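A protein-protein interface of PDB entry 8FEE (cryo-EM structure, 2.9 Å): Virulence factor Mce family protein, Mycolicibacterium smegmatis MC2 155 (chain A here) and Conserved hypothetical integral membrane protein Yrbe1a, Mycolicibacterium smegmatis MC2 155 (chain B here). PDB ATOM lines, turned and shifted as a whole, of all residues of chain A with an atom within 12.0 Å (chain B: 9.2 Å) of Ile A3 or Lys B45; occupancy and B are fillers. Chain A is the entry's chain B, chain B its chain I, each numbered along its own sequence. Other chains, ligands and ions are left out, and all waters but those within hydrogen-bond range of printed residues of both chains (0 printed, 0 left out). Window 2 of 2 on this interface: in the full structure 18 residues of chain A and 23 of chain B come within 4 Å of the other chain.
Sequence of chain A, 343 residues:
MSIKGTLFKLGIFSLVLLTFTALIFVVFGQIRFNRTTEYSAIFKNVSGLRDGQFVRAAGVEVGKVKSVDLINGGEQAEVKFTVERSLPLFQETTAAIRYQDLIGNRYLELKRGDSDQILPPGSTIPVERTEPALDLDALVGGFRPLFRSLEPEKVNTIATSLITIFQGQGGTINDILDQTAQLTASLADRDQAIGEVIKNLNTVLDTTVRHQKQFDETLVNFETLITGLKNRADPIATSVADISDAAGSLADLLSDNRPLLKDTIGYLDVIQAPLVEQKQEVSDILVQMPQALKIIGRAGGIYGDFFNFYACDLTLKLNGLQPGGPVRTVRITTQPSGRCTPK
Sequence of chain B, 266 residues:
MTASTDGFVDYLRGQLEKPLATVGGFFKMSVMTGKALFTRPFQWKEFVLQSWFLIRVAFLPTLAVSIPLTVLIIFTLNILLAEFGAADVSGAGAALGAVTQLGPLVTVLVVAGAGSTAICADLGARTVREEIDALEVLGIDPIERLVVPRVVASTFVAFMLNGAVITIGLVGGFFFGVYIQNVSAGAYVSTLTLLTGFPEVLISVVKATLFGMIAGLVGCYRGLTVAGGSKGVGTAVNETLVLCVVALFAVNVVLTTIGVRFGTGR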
ATOM      1  N   ILE A   3     -10.835  12.684  10.744  1.00  0.00           N
ATOM      2  CA  ILE A   3     -11.115  13.577   9.628  1.00  0.00           C
ATOM      3  C   ILE A   3     -11.219  12.760   8.343  1.00  0.00           C
ATOM      4  O   ILE A   3     -11.775  13.220   7.348  1.00  0.00           O
ATOM      5  CB  ILE A   3     -10.040  14.684   9.517  1.00  0.00           C
ATOM      6  CG1 ILE A   3     -10.523  15.828   8.622  1.00  0.00           C
ATOM      7  CG2 ILE A   3      -8.727  14.116   9.001  1.00  0.00           C
ATOM      8  CD1 ILE A   3      -9.566  16.997   8.553  1.00  0.00           C
ATOM      9  N   LYS A   4     -10.683  11.536   8.384  1.00  0.00           N
ATOM     10  CA  LYS A   4     -10.710  10.660   7.215  1.00  0.00           C
ATOM     11  C   LYS A   4     -12.142  10.332   6.804  1.00  0.00           C
ATOM     12  O   LYS A   4     -12.501  10.429   5.623  1.00  0.00           O
ATOM     13  CB  LYS A   4      -9.926   9.380   7.510  1.00  0.00           C
ATOM     14  CG  LYS A   4      -9.586   8.551   6.283  1.00  0.00           C
ATOM     15  CD  LYS A   4      -8.453   9.182   5.493  1.00  0.00           C
ATOM     16  CE  LYS A   4      -7.920   8.233   4.432  1.00  0.00           C
ATOM     17  NZ  LYS A   4      -8.995   7.765   3.515  1.00  0.00           N
ATOM     18  N   GLY A   5     -12.976   9.945   7.770  1.00  0.00           N
ATOM     19  CA  GLY A   5     -14.378   9.704   7.473  1.00  0.00           C
ATOM     20  C   GLY A   5     -15.109  10.963   7.050  1.00  0.00           C
ATOM     21  O   GLY A   5     -15.930  10.934   6.128  1.00  0.00           O
ATOM     22  N   THR A   6     -14.819  12.086   7.713  1.00  0.00           N
ATOM     23  CA  THR A   6     -15.398  13.361   7.300  1.00  0.00           C
ATOM     24  C   THR A   6     -14.944  13.728   5.893  1.00  0.00           C
ATOM     25  O   THR A   6     -15.740  14.224   5.085  1.00  0.00           O
ATOM     26  CB  THR A   6     -15.016  14.457   8.297  1.00  0.00           C
ATOM     27  OG1 THR A   6     -15.655  14.204   9.554  1.00  0.00           O
ATOM     28  CG2 THR A   6     -15.444  15.827   7.791  1.00  0.00           C
ATOM     29  N   LEU A   7     -13.672  13.474   5.578  1.00  0.00           N
ATOM     30  CA  LEU A   7     -13.168  13.736   4.234  1.00  0.00           C
ATOM     31  C   LEU A   7     -13.911  12.902   3.199  1.00  0.00           C
ATOM     32  O   LEU A   7     -14.312  13.414   2.149  1.00  0.00           O
ATOM     33  CB  LEU A   7     -11.666  13.459   4.171  1.00  0.00           C
ATOM     34  CG  LEU A   7     -10.988  13.726   2.827  1.00  0.00           C
ATOM     35  CD1 LEU A   7     -11.086  15.198   2.462  1.00  0.00           C
ATOM     36  CD2 LEU A   7      -9.538  13.271   2.856  1.00  0.00           C
ATOM     37  N   PHE A   8     -14.102  11.608   3.478  1.00  0.00           N
ATOM     38  CA  PHE A   8     -14.819  10.747   2.540  1.00  0.00           C
ATOM     39  C   PHE A   8     -16.265  11.195   2.357  1.00  0.00           C
ATOM     40  O   PHE A   8     -16.773  11.229   1.229  1.00  0.00           O
ATOM     41  CB  PHE A   8     -14.765   9.295   3.011  1.00  0.00           C
ATOM     42  CG  PHE A   8     -13.604   8.520   2.458  1.00  0.00           C
ATOM     43  CD1 PHE A   8     -13.038   8.868   1.243  1.00  0.00           C
ATOM     44  CD2 PHE A   8     -13.081   7.440   3.151  1.00  0.00           C
ATOM     45  CE1 PHE A   8     -11.969   8.157   0.731  1.00  0.00           C
ATOM     46  CE2 PHE A   8     -12.013   6.725   2.643  1.00  0.00           C
ATOM     47  CZ  PHE A   8     -11.457   7.084   1.431  1.00  0.00           C
ATOM     48  N   LYS A   9     -16.947  11.535   3.456  1.00  0.00           N
ATOM     49  CA  LYS A   9     -18.340  11.964   3.363  1.00  0.00           C
ATOM     50  C   LYS A   9     -18.463  13.253   2.561  1.00  0.00           C
ATOM     51  O   LYS A   9     -19.337  13.378   1.691  1.00  0.00           O
ATOM     52  CB  LYS A   9     -18.934  12.140   4.761  1.00  0.00           C
ATOM     53  CG  LYS A   9     -19.056  10.851   5.556  1.00  0.00           C
ATOM     54  CD  LYS A   9     -19.603  11.116   6.949  1.00  0.00           C
ATOM     55  CE  LYS A   9     -19.793   9.825   7.725  1.00  0.00           C
ATOM     56  NZ  LYS A   9     -20.394  10.068   9.064  1.00  0.00           N
ATOM     57  N   LEU A  10     -17.591  14.225   2.841  1.00  0.00           N
ATOM     58  CA  LEU A  10     -17.616  15.480   2.101  1.00  0.00           C
ATOM     59  C   LEU A  10     -17.293  15.256   0.631  1.00  0.00           C
ATOM     60  O   LEU A  10     -17.922  15.859  -0.244  1.00  0.00           O
ATOM     61  CB  LEU A  10     -16.634  16.474   2.717  1.00  0.00           C
ATOM     62  CG  LEU A  10     -16.554  17.842   2.041  1.00  0.00           C
ATOM     63  CD1 LEU A  10     -17.911  18.520   2.037  1.00  0.00           C
ATOM     64  CD2 LEU A  10     -15.512  18.716   2.714  1.00  0.00           C
ATOM     65  N   GLY A  11     -16.324  14.386   0.341  1.00  0.00           N
ATOM     66  CA  GLY A  11     -15.994  14.089  -1.042  1.00  0.00           C
ATOM     67  C   GLY A  11     -17.156  13.479  -1.800  1.00  0.00           C
ATOM     68  O   GLY A  11     -17.457  13.884  -2.923  1.00  0.00           O
ATOM     69  N   ILE A  12     -17.840  12.511  -1.185  1.00  0.00           N
ATOM     70  CA  ILE A  12     -18.969  11.861  -1.848  1.00  0.00           C
ATOM     71  C   ILE A  12     -20.106  12.853  -2.072  1.00  0.00           C
ATOM     72  O   ILE A  12     -20.672  12.935  -3.173  1.00  0.00           O
ATOM     73  CB  ILE A  12     -19.435  10.640  -1.037  1.00  0.00           C
ATOM     74  CG1 ILE A  12     -18.363   9.549  -1.052  1.00  0.00           C
ATOM     75  CG2 ILE A  12     -20.751  10.103  -1.580  1.00  0.00           C
ATOM     76  CD1 ILE A  12     -18.729   8.325  -0.245  1.00  0.00           C
ATOM     77  N   PHE B  42      -3.720  28.165   3.118  1.00  0.00           N
ATOM     78  CA  PHE B  42      -5.100  27.787   3.381  1.00  0.00           C
ATOM     79  C   PHE B  42      -5.174  26.643   4.386  1.00  0.00           C
ATOM     80  O   PHE B  42      -4.251  25.834   4.513  1.00  0.00           O
ATOM     81  CB  PHE B  42      -5.793  27.382   2.079  1.00  0.00           C
ATOM     82  CG  PHE B  42      -7.290  27.405   2.155  1.00  0.00           C
ATOM     83  CD1 PHE B  42      -7.974  28.606   2.217  1.00  0.00           C
ATOM     84  CD2 PHE B  42      -8.014  26.226   2.154  1.00  0.00           C
ATOM     85  CE1 PHE B  42      -9.350  28.630   2.284  1.00  0.00           C
ATOM     86  CE2 PHE B  42      -9.391  26.246   2.220  1.00  0.00           C
ATOM     87  CZ  PHE B  42     -10.061  27.449   2.285  1.00  0.00           C
ATOM     88  N   GLN B  43      -6.293  26.588   5.106  1.00  0.00           N
ATOM     89  CA  GLN B  43      -6.538  25.575   6.130  1.00  0.00           C
ATOM     90  C   GLN B  43      -7.455  24.511   5.535  1.00  0.00           C
ATOM     91  O   GLN B  43      -8.674  24.687   5.487  1.00  0.00           O
ATOM     92  CB  GLN B  43      -7.151  26.206   7.376  1.00  0.00           C
ATOM     93  CG  GLN B  43      -6.331  27.339   7.973  1.00  0.00           C
ATOM     94  CD  GLN B  43      -5.067  26.854   8.657  1.00  0.00           C
ATOM     95  OE1 GLN B  43      -4.947  25.680   9.005  1.00  0.00           O
ATOM     96  NE2 GLN B  43      -4.117  27.761   8.853  1.00  0.00           N
ATOM     97  N   TRP B  44      -6.864  23.405   5.073  1.00  0.00           N
ATOM     98  CA  TRP B  44      -7.662  22.333   4.487  1.00  0.00           C
ATOM     99  C   TRP B  44      -8.542  21.649   5.527  1.00  0.00           C
ATOM    100  O   TRP B  44      -9.708  21.341   5.254  1.00  0.00           O
ATOM    101  CB  TRP B  44      -6.752  21.311   3.807  1.00  0.00           C
ATOM    102  CG  TRP B  44      -6.107  21.821   2.560  1.00  0.00           C
ATOM    103  CD1 TRP B  44      -4.806  22.198   2.404  1.00  0.00           C
ATOM    104  CD2 TRP B  44      -6.736  22.010   1.287  1.00  0.00           C
ATOM    105  NE1 TRP B  44      -4.585  22.612   1.112  1.00  0.00           N
ATOM    106  CE2 TRP B  44      -5.755  22.506   0.406  1.00  0.00           C
ATOM    107  CE3 TRP B  44      -8.034  21.809   0.807  1.00  0.00           C
ATOM    108  CZ2 TRP B  44      -6.029  22.804  -0.926  1.00  0.00           C
ATOM    109  CZ3 TRP B  44      -8.305  22.104  -0.515  1.00  0.00           C
ATOM    110  CH2 TRP B  44      -7.307  22.597  -1.367  1.00  0.00           C
ATOM    111  N   LYS B  45      -8.003  21.406   6.725  1.00  0.00           N
ATOM    112  CA  LYS B  45      -8.740  20.657   7.739  1.00  0.00           C
ATOM    113  C   LYS B  45      -9.980  21.412   8.199  1.00  0.00           C
ATOM    114  O   LYS B  45     -11.083  20.851   8.246  1.00  0.00           O
ATOM    115  CB  LYS B  45      -7.826  20.350   8.925  1.00  0.00           C
ATOM    116  CG  LYS B  45      -6.530  19.654   8.546  1.00  0.00           C
ATOM    117  CD  LYS B  45      -5.658  19.410   9.766  1.00  0.00           C
ATOM    118  CE  LYS B  45      -4.354  18.724   9.389  1.00  0.00           C
ATOM    119  NZ  LYS B  45      -4.584  17.384   8.787  1.00  0.00           N
ATOM    120  N   GLU B  46      -9.820  22.694   8.534  1.00  0.00           N
ATOM    121  CA  GLU B  46     -10.954  23.477   9.010  1.00  0.00           C
ATOM    122  C   GLU B  46     -11.969  23.704   7.900  1.00  0.00           C
ATOM    123  O   GLU B  46     -13.178  23.721   8.155  1.00  0.00           O
ATOM    124  CB  GLU B  46     -10.473  24.808   9.584  1.00  0.00           C
ATOM    125  CG  GLU B  46     -11.497  25.520  10.459  1.00  0.00           C
ATOM    126  CD  GLU B  46     -11.789  24.790  11.760  1.00  0.00           C
ATOM    127  OE1 GLU B  46     -10.990  23.916  12.159  1.00  0.00           O
ATOM    128  OE2 GLU B  46     -12.824  25.094  12.389  1.00  0.00           O
ATOM    129  N   PHE B  47     -11.498  23.876   6.662  1.00  0.00           N
ATOM    130  CA  PHE B  47     -12.412  23.993   5.530  1.00  0.00           C
ATOM    131  C   PHE B  47     -13.250  22.732   5.366  1.00  0.00           C
ATOM    132  O   PHE B  47     -14.468  22.809   5.173  1.00  0.00           O
ATOM    133  CB  PHE B  47     -11.632  24.289   4.249  1.00  0.00           C
ATOM    134  CG  PHE B  47     -12.424  24.070   2.994  1.00  0.00           C
ATOM    135  CD1 PHE B  47     -13.445  24.936   2.641  1.00  0.00           C
ATOM    136  CD2 PHE B  47     -12.140  23.003   2.159  1.00  0.00           C
ATOM    137  CE1 PHE B  47     -14.174  24.733   1.487  1.00  0.00           C
ATOM    138  CE2 PHE B  47     -12.864  22.798   1.002  1.00  0.00           C
ATOM    139  CZ  PHE B  47     -13.883  23.665   0.665  1.00  0.00           C
ATOM    140  N   VAL B  48     -12.616  21.560   5.446  1.00  0.00           N
ATOM    141  CA  VAL B  48     -13.351  20.302   5.315  1.00  0.00           C
ATOM    142  C   VAL B  48     -14.373  20.164   6.438  1.00  0.00           C
ATOM    143  O   VAL B  48     -15.538  19.805   6.206  1.00  0.00           O
ATOM    144  CB  VAL B  48     -12.377  19.110   5.287  1.00  0.00           C
ATOM    145  CG1 VAL B  48     -13.122  17.805   5.504  1.00  0.00           C
ATOM    146  CG2 VAL B  48     -11.630  19.073   3.967  1.00  0.00           C
ATOM    147  N   LEU B  49     -13.954  20.456   7.673  1.00  0.00           N
ATOM    148  CA  LEU B  49     -14.846  20.290   8.816  1.00  0.00           C
ATOM    149  C   LEU B  49     -16.040  21.234   8.726  1.00  0.00           C
ATOM    150  O   LEU B  49     -17.186  20.824   8.945  1.00  0.00           O
ATOM    151  CB  LEU B  49     -14.079  20.508  10.120  1.00  0.00           C
ATOM    152  CG  LEU B  49     -13.000  19.476  10.451  1.00  0.00           C
ATOM    153  CD1 LEU B  49     -12.273  19.852  11.729  1.00  0.00           C
ATOM    154  CD2 LEU B  49     -13.606  18.089  10.565  1.00  0.00           C
ATOM    155  N   GLN B  50     -15.793  22.501   8.386  1.00  0.00           N
ATOM    156  CA  GLN B  50     -16.888  23.457   8.277  1.00  0.00           C
ATOM    157  C   GLN B  50     -17.788  23.155   7.089  1.00  0.00           C
ATOM    158  O   GLN B  50     -19.002  23.366   7.175  1.00  0.00           O
ATOM    159  CB  GLN B  50     -16.339  24.878   8.184  1.00  0.00           C
ATOM    160  CG  GLN B  50     -15.762  25.382   9.488  1.00  0.00           C
ATOM    161  CD  GLN B  50     -16.746  25.261  10.634  1.00  0.00           C
ATOM    162  OE1 GLN B  50     -17.870  25.754  10.554  1.00  0.00           O
ATOM    163  NE2 GLN B  50     -16.328  24.597  11.705  1.00  0.00           N
ATOM    164  N   SER B  51     -17.228  22.660   5.981  1.00  0.00           N
ATOM    165  CA  SER B  51     -18.060  22.260   4.851  1.00  0.00           C
ATOM    166  C   SER B  51     -19.003  21.133   5.245  1.00  0.00           C
ATOM    167  O   SER B  51     -20.204  21.186   4.956  1.00  0.00           O
ATOM    168  CB  SER B  51     -17.181  21.832   3.676  1.00  0.00           C
ATOM    169  OG  SER B  51     -16.340  22.886   3.247  1.00  0.00           O
ATOM    170  N   TRP B  52     -18.478  20.107   5.920  1.00  0.00           N
ATOM    171  CA  TRP B  52     -19.339  19.001   6.329  1.00  0.00           C
ATOM    172  C   TRP B  52     -20.375  19.453   7.350  1.00  0.00           C
ATOM    173  O   TRP B  52     -21.527  19.005   7.312  1.00  0.00           O
ATOM    174  CB  TRP B  52     -18.509  17.849   6.886  1.00  0.00           C
ATOM    175  CG  TRP B  52     -19.362  16.735   7.398  1.00  0.00           C
ATOM    176  CD1 TRP B  52     -19.494  16.336   8.694  1.00  0.00           C
ATOM    177  CD2 TRP B  52     -20.227  15.892   6.629  1.00  0.00           C
ATOM    178  NE1 TRP B  52     -20.376  15.287   8.779  1.00  0.00           N
ATOM    179  CE2 TRP B  52     -20.842  14.996   7.524  1.00  0.00           C
ATOM    180  CE3 TRP B  52     -20.536  15.803   5.268  1.00  0.00           C
ATOM    181  CZ2 TRP B  52     -21.746  14.026   7.105  1.00  0.00           C
ATOM    182  CZ3 TRP B  52     -21.434  14.839   4.854  1.00  0.00           C
ATOM    183  CH2 TRP B  52     -22.028  13.963   5.768  1.00  0.00           C
ATOM    184  N   PHE B  53     -19.983  20.333   8.275  1.00  0.00           N
ATOM    185  CA  PHE B  53     -20.921  20.832   9.277  1.00  0.00           C
ATOM    186  C   PHE B  53     -22.059  21.609   8.622  1.00  0.00           C
ATOM    187  O   PHE B  53     -23.240  21.374   8.914  1.00  0.00           O
ATOM    188  CB  PHE B  53     -20.176  21.695  10.294  1.00  0.00           C
ATOM    189  CG  PHE B  53     -21.074  22.494  11.190  1.00  0.00           C
ATOM    190  CD1 PHE B  53     -21.725  21.892  12.252  1.00  0.00           C
ATOM    191  CD2 PHE B  53     -21.248  23.853  10.987  1.00  0.00           C
ATOM    192  CE1 PHE B  53     -22.548  22.625  13.082  1.00  0.00           C
ATOM    193  CE2 PHE B  53     -22.067  24.589  11.813  1.00  0.00           C
ATOM    194  CZ  PHE B  53     -22.718  23.975  12.863  1.00  0.00           C
ATOM    195  N   ARG B 145      -7.179  31.571  10.698  1.00  0.00           N
ATOM    196  CA  ARG B 145      -7.395  30.206  11.159  1.00  0.00           C
ATOM    197  C   ARG B 145      -8.867  29.812  11.152  1.00  0.00           C
ATOM    198  O   ARG B 145      -9.185  28.639  10.924  1.00  0.00           O
ATOM    199  CB  ARG B 145      -6.802  30.027  12.558  1.00  0.00           C
ATOM    200  CG  ARG B 145      -6.905  28.612  13.106  1.00  0.00           C
ATOM    201  CD  ARG B 145      -5.820  28.332  14.128  1.00  0.00           C
ATOM    202  NE  ARG B 145      -4.490  28.473  13.550  1.00  0.00           N
ATOM    203  CZ  ARG B 145      -3.796  27.478  13.013  1.00  0.00           C
ATOM    204  NH1 ARG B 145      -4.274  26.246  12.976  1.00  0.00           N
ATOM    205  NH2 ARG B 145      -2.594  27.726  12.504  1.00  0.00           N
ATOM    206  N   PRO B 149     -11.587  29.613   6.259  1.00  0.00           N
ATOM    207  CA  PRO B 149     -12.201  28.329   5.887  1.00  0.00           C
ATOM    208  C   PRO B 149     -13.709  28.331   6.032  1.00  0.00           C
ATOM    209  O   PRO B 149     -14.396  27.681   5.238  1.00  0.00           O
ATOM    210  CB  PRO B 149     -11.538  27.329   6.841  1.00  0.00           C
ATOM    211  CG  PRO B 149     -11.119  28.138   7.990  1.00  0.00           C
ATOM    212  CD  PRO B 149     -10.684  29.438   7.413  1.00  0.00           C
ATOM    213  N   ARG B 150     -14.245  29.058   7.015  1.00  0.00           N
ATOM    214  CA  ARG B 150     -15.693  29.124   7.188  1.00  0.00           C
ATOM    215  C   ARG B 150     -16.366  29.792   5.994  1.00  0.00           C
ATOM    216  O   ARG B 150     -17.387  29.304   5.500  1.00  0.00           O
ATOM    217  CB  ARG B 150     -16.028  29.872   8.478  1.00  0.00           C
ATOM    218  CG  ARG B 150     -16.762  29.045   9.520  1.00  0.00           C
ATOM    219  CD  ARG B 150     -16.359  29.459  10.925  1.00  0.00           C
ATOM    220  NE  ARG B 150     -15.042  28.949  11.282  1.00  0.00           N
ATOM    221  CZ  ARG B 150     -14.831  27.960  12.140  1.00  0.00           C
ATOM    222  NH1 ARG B 150     -15.829  27.381  12.785  1.00  0.00           N
ATOM    223  NH2 ARG B 150     -13.587  27.546  12.358  1.00  0.00           N
ATOM    224  N   ALA B 153     -16.071  27.481   2.924  1.00  0.00           N
ATOM    225  CA  ALA B 153     -17.017  26.384   3.081  1.00  0.00           C
ATOM    226  C   ALA B 153     -18.446  26.845   2.834  1.00  0.00           C
ATOM    227  O   ALA B 153     -19.234  26.127   2.212  1.00  0.00           O
ATOM    228  CB  ALA B 153     -16.886  25.780   4.477  1.00  0.00           C
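The backbone carbonyl oxygen (O) of Phe B47 lies within hydrogen-bond range of the side-chain hydroxyl (OG) of Ser B51 (2.7 Å).
Lys B45 touches Ile A3. Thr A6 touches Val B48 (CG2 to CG1, 3.8 Å). Thr A6 touches Trp B52 (CG2 to CB, 3.8 Å). Trp B52 touches Lys A9 (CZ2 to CD, 3.6 Å). CD2 of Leu A10 touches O of Val B48 (3.7 Å). CD2 of Leu A10 touches CB of Ser B51, at 3.7 Å.
Of chain B, only Lys B45 (3.8 Å) comes within 4 Å of Ile A3. Of the printed residues of chain A, Lys B45 touches Ile A3. Gly A5 touches none of the printed residues of chain B. Thr A6 touches two residues of chain B. No residue of chain A comes within 4 Å of Gln B43. No residue of chain A comes within 4 Å of Glu B46. Val B48 touches just these residues of chain A: Thr A6 and Leu A10. No residue of chain A comes within 4 Å of Leu B49. Of the printed residues of chain B, Leu A10 touches Val B48 and Ser B51. Of the printed residues of chain A, Trp B52 touches Thr A6 (3.8 Å) and Lys A9 (3.6 Å). Of the printed residues of chain B, Lys A9 touches Trp B52 (3.6 Å). Of the printed residues of chain A, Ser B51 touches Leu A10. Trp B44 touches none of the printed residues of chain A. Phe B53 touches none of the printed residues of chain A. The nearest residue of chain A that does not touch Lys B45 is Thr A6 (6.7 Å). The nearest printed residue of chain A that does not touch Ser B51 is Thr A6 (6.9 Å).
Of the 10 printed residues of chain A, 4 touch a printed residue of chain B. Printed residues of chain A that touch a printed residue of chain B: Ile A3, Thr A6, Lys A9 and Leu A10. Hydrophobic or aromatic side chains of chain A that line the printed part of chain B: Ile A3 and Leu A10. Among the printed residues, 6 pairs touch across the chains.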
